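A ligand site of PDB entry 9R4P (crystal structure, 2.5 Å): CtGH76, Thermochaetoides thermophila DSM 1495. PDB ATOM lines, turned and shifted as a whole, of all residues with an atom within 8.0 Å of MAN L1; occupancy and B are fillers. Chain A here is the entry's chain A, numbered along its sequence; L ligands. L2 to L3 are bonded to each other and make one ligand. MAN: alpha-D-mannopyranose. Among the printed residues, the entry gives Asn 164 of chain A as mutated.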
ATOM      1  N   ARG A 103      14.651  23.013 -16.941  1.00  0.00           N
ATOM      2  CA  ARG A 103      15.440  22.593 -15.792  1.00  0.00           C
ATOM      3  C   ARG A 103      16.728  21.987 -16.330  1.00  0.00           C
ATOM      4  O   ARG A 103      16.760  21.478 -17.465  1.00  0.00           O
ATOM      5  CB  ARG A 103      14.653  21.594 -14.931  1.00  0.00           C
ATOM      6  CG  ARG A 103      15.444  20.478 -14.289  1.00  0.00           C
ATOM      7  CD  ARG A 103      14.625  19.704 -13.257  1.00  0.00           C
ATOM      8  NE  ARG A 103      15.499  18.997 -12.318  1.00  0.00           N
ATOM      9  CZ  ARG A 103      15.078  18.171 -11.361  1.00  0.00           C
ATOM     10  NH1 ARG A 103      13.790  17.892 -11.216  1.00  0.00           N
ATOM     11  NH2 ARG A 103      15.968  17.629 -10.540  1.00  0.00           N
ATOM     12  N   SER A 105      19.328  18.954 -15.912  1.00  0.00           N
ATOM     13  CA  SER A 105      19.648  17.650 -15.353  1.00  0.00           C
ATOM     14  C   SER A 105      18.620  17.152 -14.344  1.00  0.00           C
ATOM     15  O   SER A 105      18.806  17.318 -13.132  1.00  0.00           O
ATOM     16  CB  SER A 105      21.043  17.679 -14.707  1.00  0.00           C
ATOM     17  OG  SER A 105      22.069  17.800 -15.685  1.00  0.00           O
ATOM     18  N   SER A 106      17.544  16.533 -14.833  1.00  0.00           N
ATOM     19  CA  SER A 106      16.514  16.008 -13.953  1.00  0.00           C
ATOM     20  C   SER A 106      17.030  14.865 -13.082  1.00  0.00           C
ATOM     21  O   SER A 106      16.375  14.517 -12.095  1.00  0.00           O
ATOM     22  CB  SER A 106      15.324  15.520 -14.782  1.00  0.00           C
ATOM     23  OG  SER A 106      14.635  16.615 -15.357  1.00  0.00           O
ATOM     24  N   ASP A 107      18.173  14.297 -13.424  1.00  0.00           N
ATOM     25  CA  ASP A 107      18.778  13.206 -12.679  1.00  0.00           C
ATOM     26  C   ASP A 107      19.728  13.682 -11.578  1.00  0.00           C
ATOM     27  O   ASP A 107      20.363  12.853 -10.932  1.00  0.00           O
ATOM     28  CB  ASP A 107      19.529  12.259 -13.636  1.00  0.00           C
ATOM     29  CG  ASP A 107      20.601  12.981 -14.449  1.00  0.00           C
ATOM     30  OD1 ASP A 107      21.532  12.306 -14.941  1.00  0.00           O
ATOM     31  OD2 ASP A 107      20.522  14.232 -14.571  1.00  0.00           O
ATOM     32  N   GLU A 108      19.849  14.987 -11.382  1.00  0.00           N
ATOM     33  CA  GLU A 108      20.629  15.555 -10.300  1.00  0.00           C
ATOM     34  C   GLU A 108      19.718  16.299  -9.341  1.00  0.00           C
ATOM     35  O   GLU A 108      18.559  16.603  -9.674  1.00  0.00           O
ATOM     36  CB  GLU A 108      21.719  16.486 -10.844  1.00  0.00           C
ATOM     37  CG  GLU A 108      22.551  15.845 -11.944  1.00  0.00           C
ATOM     38  CD  GLU A 108      23.910  15.308 -11.445  1.00  0.00           C
ATOM     39  OE1 GLU A 108      23.986  14.772 -10.312  1.00  0.00           O
ATOM     40  OE2 GLU A 108      24.893  15.402 -12.220  1.00  0.00           O
ATOM     41  N   PRO A 109      20.168  16.570  -8.115  1.00  0.00           N
ATOM     42  CA  PRO A 109      19.307  17.207  -7.121  1.00  0.00           C
ATOM     43  C   PRO A 109      18.634  18.464  -7.662  1.00  0.00           C
ATOM     44  O   PRO A 109      19.283  19.364  -8.198  1.00  0.00           O
ATOM     45  CB  PRO A 109      20.266  17.534  -5.975  1.00  0.00           C
ATOM     46  CG  PRO A 109      21.378  16.522  -6.098  1.00  0.00           C
ATOM     47  CD  PRO A 109      21.387  15.984  -7.505  1.00  0.00           C
ATOM     48  N   TRP A 110      17.314  18.510  -7.493  1.00  0.00           N
ATOM     49  CA  TRP A 110      16.539  19.657  -7.913  1.00  0.00           C
ATOM     50  C   TRP A 110      17.092  20.947  -7.335  1.00  0.00           C
ATOM     51  O   TRP A 110      17.123  21.972  -8.030  1.00  0.00           O
ATOM     52  CB  TRP A 110      15.079  19.466  -7.502  1.00  0.00           C
ATOM     53  CG  TRP A 110      14.161  20.608  -7.768  1.00  0.00           C
ATOM     54  CD1 TRP A 110      13.649  20.978  -8.982  1.00  0.00           C
ATOM     55  CD2 TRP A 110      13.625  21.526  -6.814  1.00  0.00           C
ATOM     56  NE1 TRP A 110      12.839  22.075  -8.839  1.00  0.00           N
ATOM     57  CE2 TRP A 110      12.808  22.436  -7.513  1.00  0.00           C
ATOM     58  CE3 TRP A 110      13.770  21.679  -5.433  1.00  0.00           C
ATOM     59  CZ2 TRP A 110      12.116  23.468  -6.888  1.00  0.00           C
ATOM     60  CZ3 TRP A 110      13.101  22.715  -4.799  1.00  0.00           C
ATOM     61  CH2 TRP A 110      12.274  23.598  -5.527  1.00  0.00           C
ATOM     62  N   TRP A 111      17.574  20.927  -6.078  1.00  0.00           N
ATOM     63  CA  TRP A 111      18.058  22.175  -5.486  1.00  0.00           C
ATOM     64  C   TRP A 111      19.290  22.708  -6.201  1.00  0.00           C
ATOM     65  O   TRP A 111      19.604  23.896  -6.072  1.00  0.00           O
ATOM     66  CB  TRP A 111      18.339  21.998  -4.004  1.00  0.00           C
ATOM     67  CG  TRP A 111      19.545  21.152  -3.678  1.00  0.00           C
ATOM     68  CD1 TRP A 111      19.566  19.804  -3.522  1.00  0.00           C
ATOM     69  CD2 TRP A 111      20.899  21.608  -3.468  1.00  0.00           C
ATOM     70  NE1 TRP A 111      20.835  19.382  -3.245  1.00  0.00           N
ATOM     71  CE2 TRP A 111      21.675  20.463  -3.199  1.00  0.00           C
ATOM     72  CE3 TRP A 111      21.518  22.865  -3.495  1.00  0.00           C
ATOM     73  CZ2 TRP A 111      23.045  20.525  -2.939  1.00  0.00           C
ATOM     74  CZ3 TRP A 111      22.882  22.923  -3.228  1.00  0.00           C
ATOM     75  CH2 TRP A 111      23.631  21.761  -2.950  1.00  0.00           C
ATOM     76  N   ILE A 112      20.011  21.865  -6.945  1.00  0.00           N
ATOM     77  CA  ILE A 112      21.196  22.351  -7.644  1.00  0.00           C
ATOM     78  C   ILE A 112      20.804  23.097  -8.917  1.00  0.00           C
ATOM     79  O   ILE A 112      21.516  24.006  -9.357  1.00  0.00           O
ATOM     80  CB  ILE A 112      22.168  21.193  -7.922  1.00  0.00           C
ATOM     81  CG1 ILE A 112      22.487  20.473  -6.609  1.00  0.00           C
ATOM     82  CG2 ILE A 112      23.447  21.711  -8.557  1.00  0.00           C
ATOM     83  CD1 ILE A 112      23.787  19.668  -6.627  1.00  0.00           C
ATOM     84  N   SER A 113      19.657  22.747  -9.518  1.00  0.00           N
ATOM     85  CA  SER A 113      19.081  23.602 -10.551  1.00  0.00           C
ATOM     86  C   SER A 113      18.846  25.010 -10.020  1.00  0.00           C
ATOM     87  O   SER A 113      19.053  25.993 -10.748  1.00  0.00           O
ATOM     88  CB  SER A 113      17.785  23.006 -11.078  1.00  0.00           C
ATOM     89  OG  SER A 113      18.035  22.215 -12.232  1.00  0.00           O
ATOM     90  N   LEU A 147       5.157  21.238  -6.798  1.00  0.00           N
ATOM     91  CA  LEU A 147       6.014  20.103  -7.077  1.00  0.00           C
ATOM     92  C   LEU A 147       5.246  18.800  -6.991  1.00  0.00           C
ATOM     93  O   LEU A 147       4.394  18.613  -6.109  1.00  0.00           O
ATOM     94  CB  LEU A 147       7.192  20.085  -6.099  1.00  0.00           C
ATOM     95  CG  LEU A 147       7.928  21.425  -6.098  1.00  0.00           C
ATOM     96  CD1 LEU A 147       8.883  21.521  -4.914  1.00  0.00           C
ATOM     97  CD2 LEU A 147       8.657  21.616  -7.400  1.00  0.00           C
ATOM     98  N   SER A 148       5.543  17.886  -7.923  1.00  0.00           N
ATOM     99  CA  SER A 148       4.873  16.584  -7.914  1.00  0.00           C
ATOM    100  C   SER A 148       5.214  15.801  -6.653  1.00  0.00           C
ATOM    101  O   SER A 148       4.347  15.094  -6.113  1.00  0.00           O
ATOM    102  CB  SER A 148       5.267  15.783  -9.153  1.00  0.00           C
ATOM    103  OG  SER A 148       6.636  15.995  -9.499  1.00  0.00           O
ATOM    104  N   TRP A 149       6.450  15.904  -6.168  1.00  0.00           N
ATOM    105  CA  TRP A 149       6.882  15.207  -4.963  1.00  0.00           C
ATOM    106  C   TRP A 149       6.587  15.979  -3.681  1.00  0.00           C
ATOM    107  O   TRP A 149       6.871  15.456  -2.588  1.00  0.00           O
ATOM    108  CB  TRP A 149       8.378  14.865  -5.046  1.00  0.00           C
ATOM    109  CG  TRP A 149       9.304  16.047  -4.927  1.00  0.00           C
ATOM    110  CD1 TRP A 149       9.881  16.536  -3.785  1.00  0.00           C
ATOM    111  CD2 TRP A 149       9.781  16.879  -5.997  1.00  0.00           C
ATOM    112  NE1 TRP A 149      10.675  17.623  -4.071  1.00  0.00           N
ATOM    113  CE2 TRP A 149      10.639  17.847  -5.428  1.00  0.00           C
ATOM    114  CE3 TRP A 149       9.553  16.900  -7.382  1.00  0.00           C
ATOM    115  CZ2 TRP A 149      11.270  18.830  -6.186  1.00  0.00           C
ATOM    116  CZ3 TRP A 149      10.184  17.867  -8.135  1.00  0.00           C
ATOM    117  CH2 TRP A 149      11.033  18.826  -7.535  1.00  0.00           C
ATOM    118  N   TRP A 150       6.049  17.193  -3.770  1.00  0.00           N
ATOM    119  CA  TRP A 150       5.648  17.947  -2.585  1.00  0.00           C
ATOM    120  C   TRP A 150       4.502  18.889  -2.927  1.00  0.00           C
ATOM    121  O   TRP A 150       4.661  20.116  -2.979  1.00  0.00           O
ATOM    122  CB  TRP A 150       6.821  18.726  -1.986  1.00  0.00           C
ATOM    123  CG  TRP A 150       6.559  19.137  -0.566  1.00  0.00           C
ATOM    124  CD1 TRP A 150       6.383  20.413  -0.102  1.00  0.00           C
ATOM    125  CD2 TRP A 150       6.390  18.267   0.552  1.00  0.00           C
ATOM    126  NE1 TRP A 150       6.134  20.386   1.244  1.00  0.00           N
ATOM    127  CE2 TRP A 150       6.136  19.084   1.673  1.00  0.00           C
ATOM    128  CE3 TRP A 150       6.444  16.879   0.724  1.00  0.00           C
ATOM    129  CZ2 TRP A 150       5.932  18.561   2.951  1.00  0.00           C
ATOM    130  CZ3 TRP A 150       6.246  16.361   1.996  1.00  0.00           C
ATOM    131  CH2 TRP A 150       5.994  17.199   3.088  1.00  0.00           C
ATOM    132  N   ALA A 159       9.175  23.388  -0.879  1.00  0.00           N
ATOM    133  CA  ALA A 159       9.467  21.990  -1.148  1.00  0.00           C
ATOM    134  C   ALA A 159       9.485  21.152   0.138  1.00  0.00           C
ATOM    135  O   ALA A 159       9.081  21.613   1.212  1.00  0.00           O
ATOM    136  CB  ALA A 159      10.793  21.872  -1.899  1.00  0.00           C
ATOM    137  N   ASP A 160       9.937  19.906   0.016  1.00  0.00           N
ATOM    138  CA  ASP A 160       9.949  18.910   1.080  1.00  0.00           C
ATOM    139  C   ASP A 160      11.058  19.126   2.107  1.00  0.00           C
ATOM    140  O   ASP A 160      11.123  18.372   3.081  1.00  0.00           O
ATOM    141  CB  ASP A 160      10.088  17.512   0.482  1.00  0.00           C
ATOM    142  CG  ASP A 160      11.377  17.342  -0.295  1.00  0.00           C
ATOM    143  OD1 ASP A 160      11.836  16.187  -0.455  1.00  0.00           O
ATOM    144  OD2 ASP A 160      11.969  18.366  -0.707  1.00  0.00           O
ATOM    145  N   ALA A 161      11.932  20.108   1.916  1.00  0.00           N
ATOM    146  CA  ALA A 161      12.955  20.410   2.906  1.00  0.00           C
ATOM    147  C   ALA A 161      13.165  21.911   2.953  1.00  0.00           C
ATOM    148  O   ALA A 161      12.983  22.607   1.952  1.00  0.00           O
ATOM    149  CB  ALA A 161      14.261  19.688   2.582  1.00  0.00           C
ATOM    150  N   ASN A 164      16.029  22.850   0.475  1.00  0.00           N
ATOM    151  CA  ASN A 164      15.476  22.898  -0.876  1.00  0.00           C
ATOM    152  C   ASN A 164      14.851  24.266  -1.156  1.00  0.00           C
ATOM    153  O   ASN A 164      15.272  24.988  -2.077  1.00  0.00           O
ATOM    154  CB  ASN A 164      14.414  21.806  -1.031  1.00  0.00           C
ATOM    155  CG  ASN A 164      14.992  20.532  -1.592  1.00  0.00           C
ATOM    156  OD1 ASN A 164      16.181  20.440  -1.884  1.00  0.00           O
ATOM    157  ND2 ASN A 164      14.133  19.521  -1.760  1.00  0.00           N
ATOM    158  N   GLN A 213       9.798  16.447   6.918  1.00  0.00           N
ATOM    159  CA  GLN A 213       9.018  15.256   7.239  1.00  0.00           C
ATOM    160  C   GLN A 213       9.441  14.567   8.533  1.00  0.00           C
ATOM    161  O   GLN A 213       8.649  13.811   9.096  1.00  0.00           O
ATOM    162  CB  GLN A 213       9.123  14.255   6.096  1.00  0.00           C
ATOM    163  CG  GLN A 213       8.149  14.511   4.983  1.00  0.00           C
ATOM    164  CD  GLN A 213       8.559  13.822   3.712  1.00  0.00           C
ATOM    165  OE1 GLN A 213       9.497  14.267   3.028  1.00  0.00           O
ATOM    166  NE2 GLN A 213       7.881  12.722   3.392  1.00  0.00           N
ATOM    167  N   ASP A 348      25.863  16.274  -4.430  1.00  0.00           N
ATOM    168  CA  ASP A 348      25.734  17.525  -3.676  1.00  0.00           C
ATOM    169  C   ASP A 348      27.069  18.239  -3.569  1.00  0.00           C
ATOM    170  O   ASP A 348      27.185  19.423  -3.938  1.00  0.00           O
ATOM    171  CB  ASP A 348      25.192  17.217  -2.277  1.00  0.00           C
ATOM    172  CG  ASP A 348      23.881  16.501  -2.317  1.00  0.00           C
ATOM    173  OD1 ASP A 348      23.121  16.692  -3.288  1.00  0.00           O
ATOM    174  OD2 ASP A 348      23.610  15.688  -1.410  1.00  0.00           O
HETATM  175  C1  MAN L   1      12.830  13.745  -6.732  1.00  0.00           C
HETATM  176  C2  MAN L   1      12.225  13.537  -5.308  1.00  0.00           C
HETATM  177  C3  MAN L   1      12.762  14.608  -4.311  1.00  0.00           C
HETATM  178  C4  MAN L   1      14.136  15.138  -4.725  1.00  0.00           C
HETATM  179  C5  MAN L   1      14.062  15.809  -6.133  1.00  0.00           C
HETATM  180  C6  MAN L   1      15.406  15.909  -6.824  1.00  0.00           C
HETATM  181  O1  MAN L   1      11.887  13.175  -7.645  1.00  0.00           O
HETATM  182  O2  MAN L   1      12.584  12.260  -4.771  1.00  0.00           O
HETATM  183  O3  MAN L   1      12.805  14.115  -2.949  1.00  0.00           O
HETATM  184  O4  MAN L   1      14.602  16.086  -3.740  1.00  0.00           O
HETATM  185  O5  MAN L   1      13.138  15.099  -7.032  1.00  0.00           O
HETATM  186  O6  MAN L   1      16.266  16.715  -6.011  1.00  0.00           O
HETATM  187  C1  MAN L   2      19.623  18.879   0.555  1.00  0.00           C
HETATM  188  C2  MAN L   2      20.223  20.106  -0.188  1.00  0.00           C
HETATM  189  C3  MAN L   2      21.605  20.509   0.319  1.00  0.00           C
HETATM  190  C4  MAN L   2      22.249  19.409   1.186  1.00  0.00           C
HETATM  191  C5  MAN L   2      21.922  18.026   0.571  1.00  0.00           C
HETATM  192  C6  MAN L   2      22.619  16.873   1.253  1.00  0.00           C
HETATM  193  O1  MAN L   2      18.434  18.532  -0.145  1.00  0.00           O
HETATM  194  O2  MAN L   2      19.425  21.287   0.009  1.00  0.00           O
HETATM  195  O3  MAN L   2      21.531  21.768   1.007  1.00  0.00           O
HETATM  196  O4  MAN L   2      23.649  19.616   1.221  1.00  0.00           O
HETATM  197  O5  MAN L   2      20.495  17.774   0.696  1.00  0.00           O
HETATM  198  O6  MAN L   2      22.423  17.037   2.641  1.00  0.00           O
HETATM  199  C1  MAN L   3      23.358  16.275   3.447  1.00  0.00           C
HETATM  200  C2  MAN L   3      23.220  16.892   4.864  1.00  0.00           C
HETATM  201  C3  MAN L   3      23.959  18.239   4.888  1.00  0.00           C
HETATM  202  C4  MAN L   3      25.423  18.080   4.455  1.00  0.00           C
HETATM  203  C5  MAN L   3      25.516  17.495   3.034  1.00  0.00           C
HETATM  204  C6  MAN L   3      26.985  17.191   2.658  1.00  0.00           C
HETATM  205  O2  MAN L   3      23.746  16.049   5.903  1.00  0.00           O
HETATM  206  O3  MAN L   3      23.871  18.912   6.160  1.00  0.00           O
HETATM  207  O4  MAN L   3      26.068  19.356   4.466  1.00  0.00           O
HETATM  208  O5  MAN L   3      24.724  16.265   2.946  1.00  0.00           O
HETATM  209  O6  MAN L   3      27.059  16.399   1.476  1.00  0.00           O
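Pro 109 touches MAN L1. Trp 149 touches MAN L1. Asn 164 touches MAN L1 (ND2 to O4, 3.99 Å). Hydrophobic or aromatic side chains within 4 Å of MAN L1: Trp 110 and Trp 149. Five residues have an atom within 4 Å of MAN L1: Pro 109, Trp 110, Trp 149, Asp 160 and Asn 164.
N of Trp 110 sits at hydrogen-bond distance from O6 of MAN L1 (2.6 Å). O3 of MAN L1 is in hydrogen-bond range of OD1 of Asp 160 (3.4 Å). OD1 of Asn 164 is in hydrogen-bond range of O1 of MAN L2, at 3.4 Å.
OD2 of Asp 160 lies within hydrogen-bond range of ND2 of Asn 164, 2.7 Å away.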
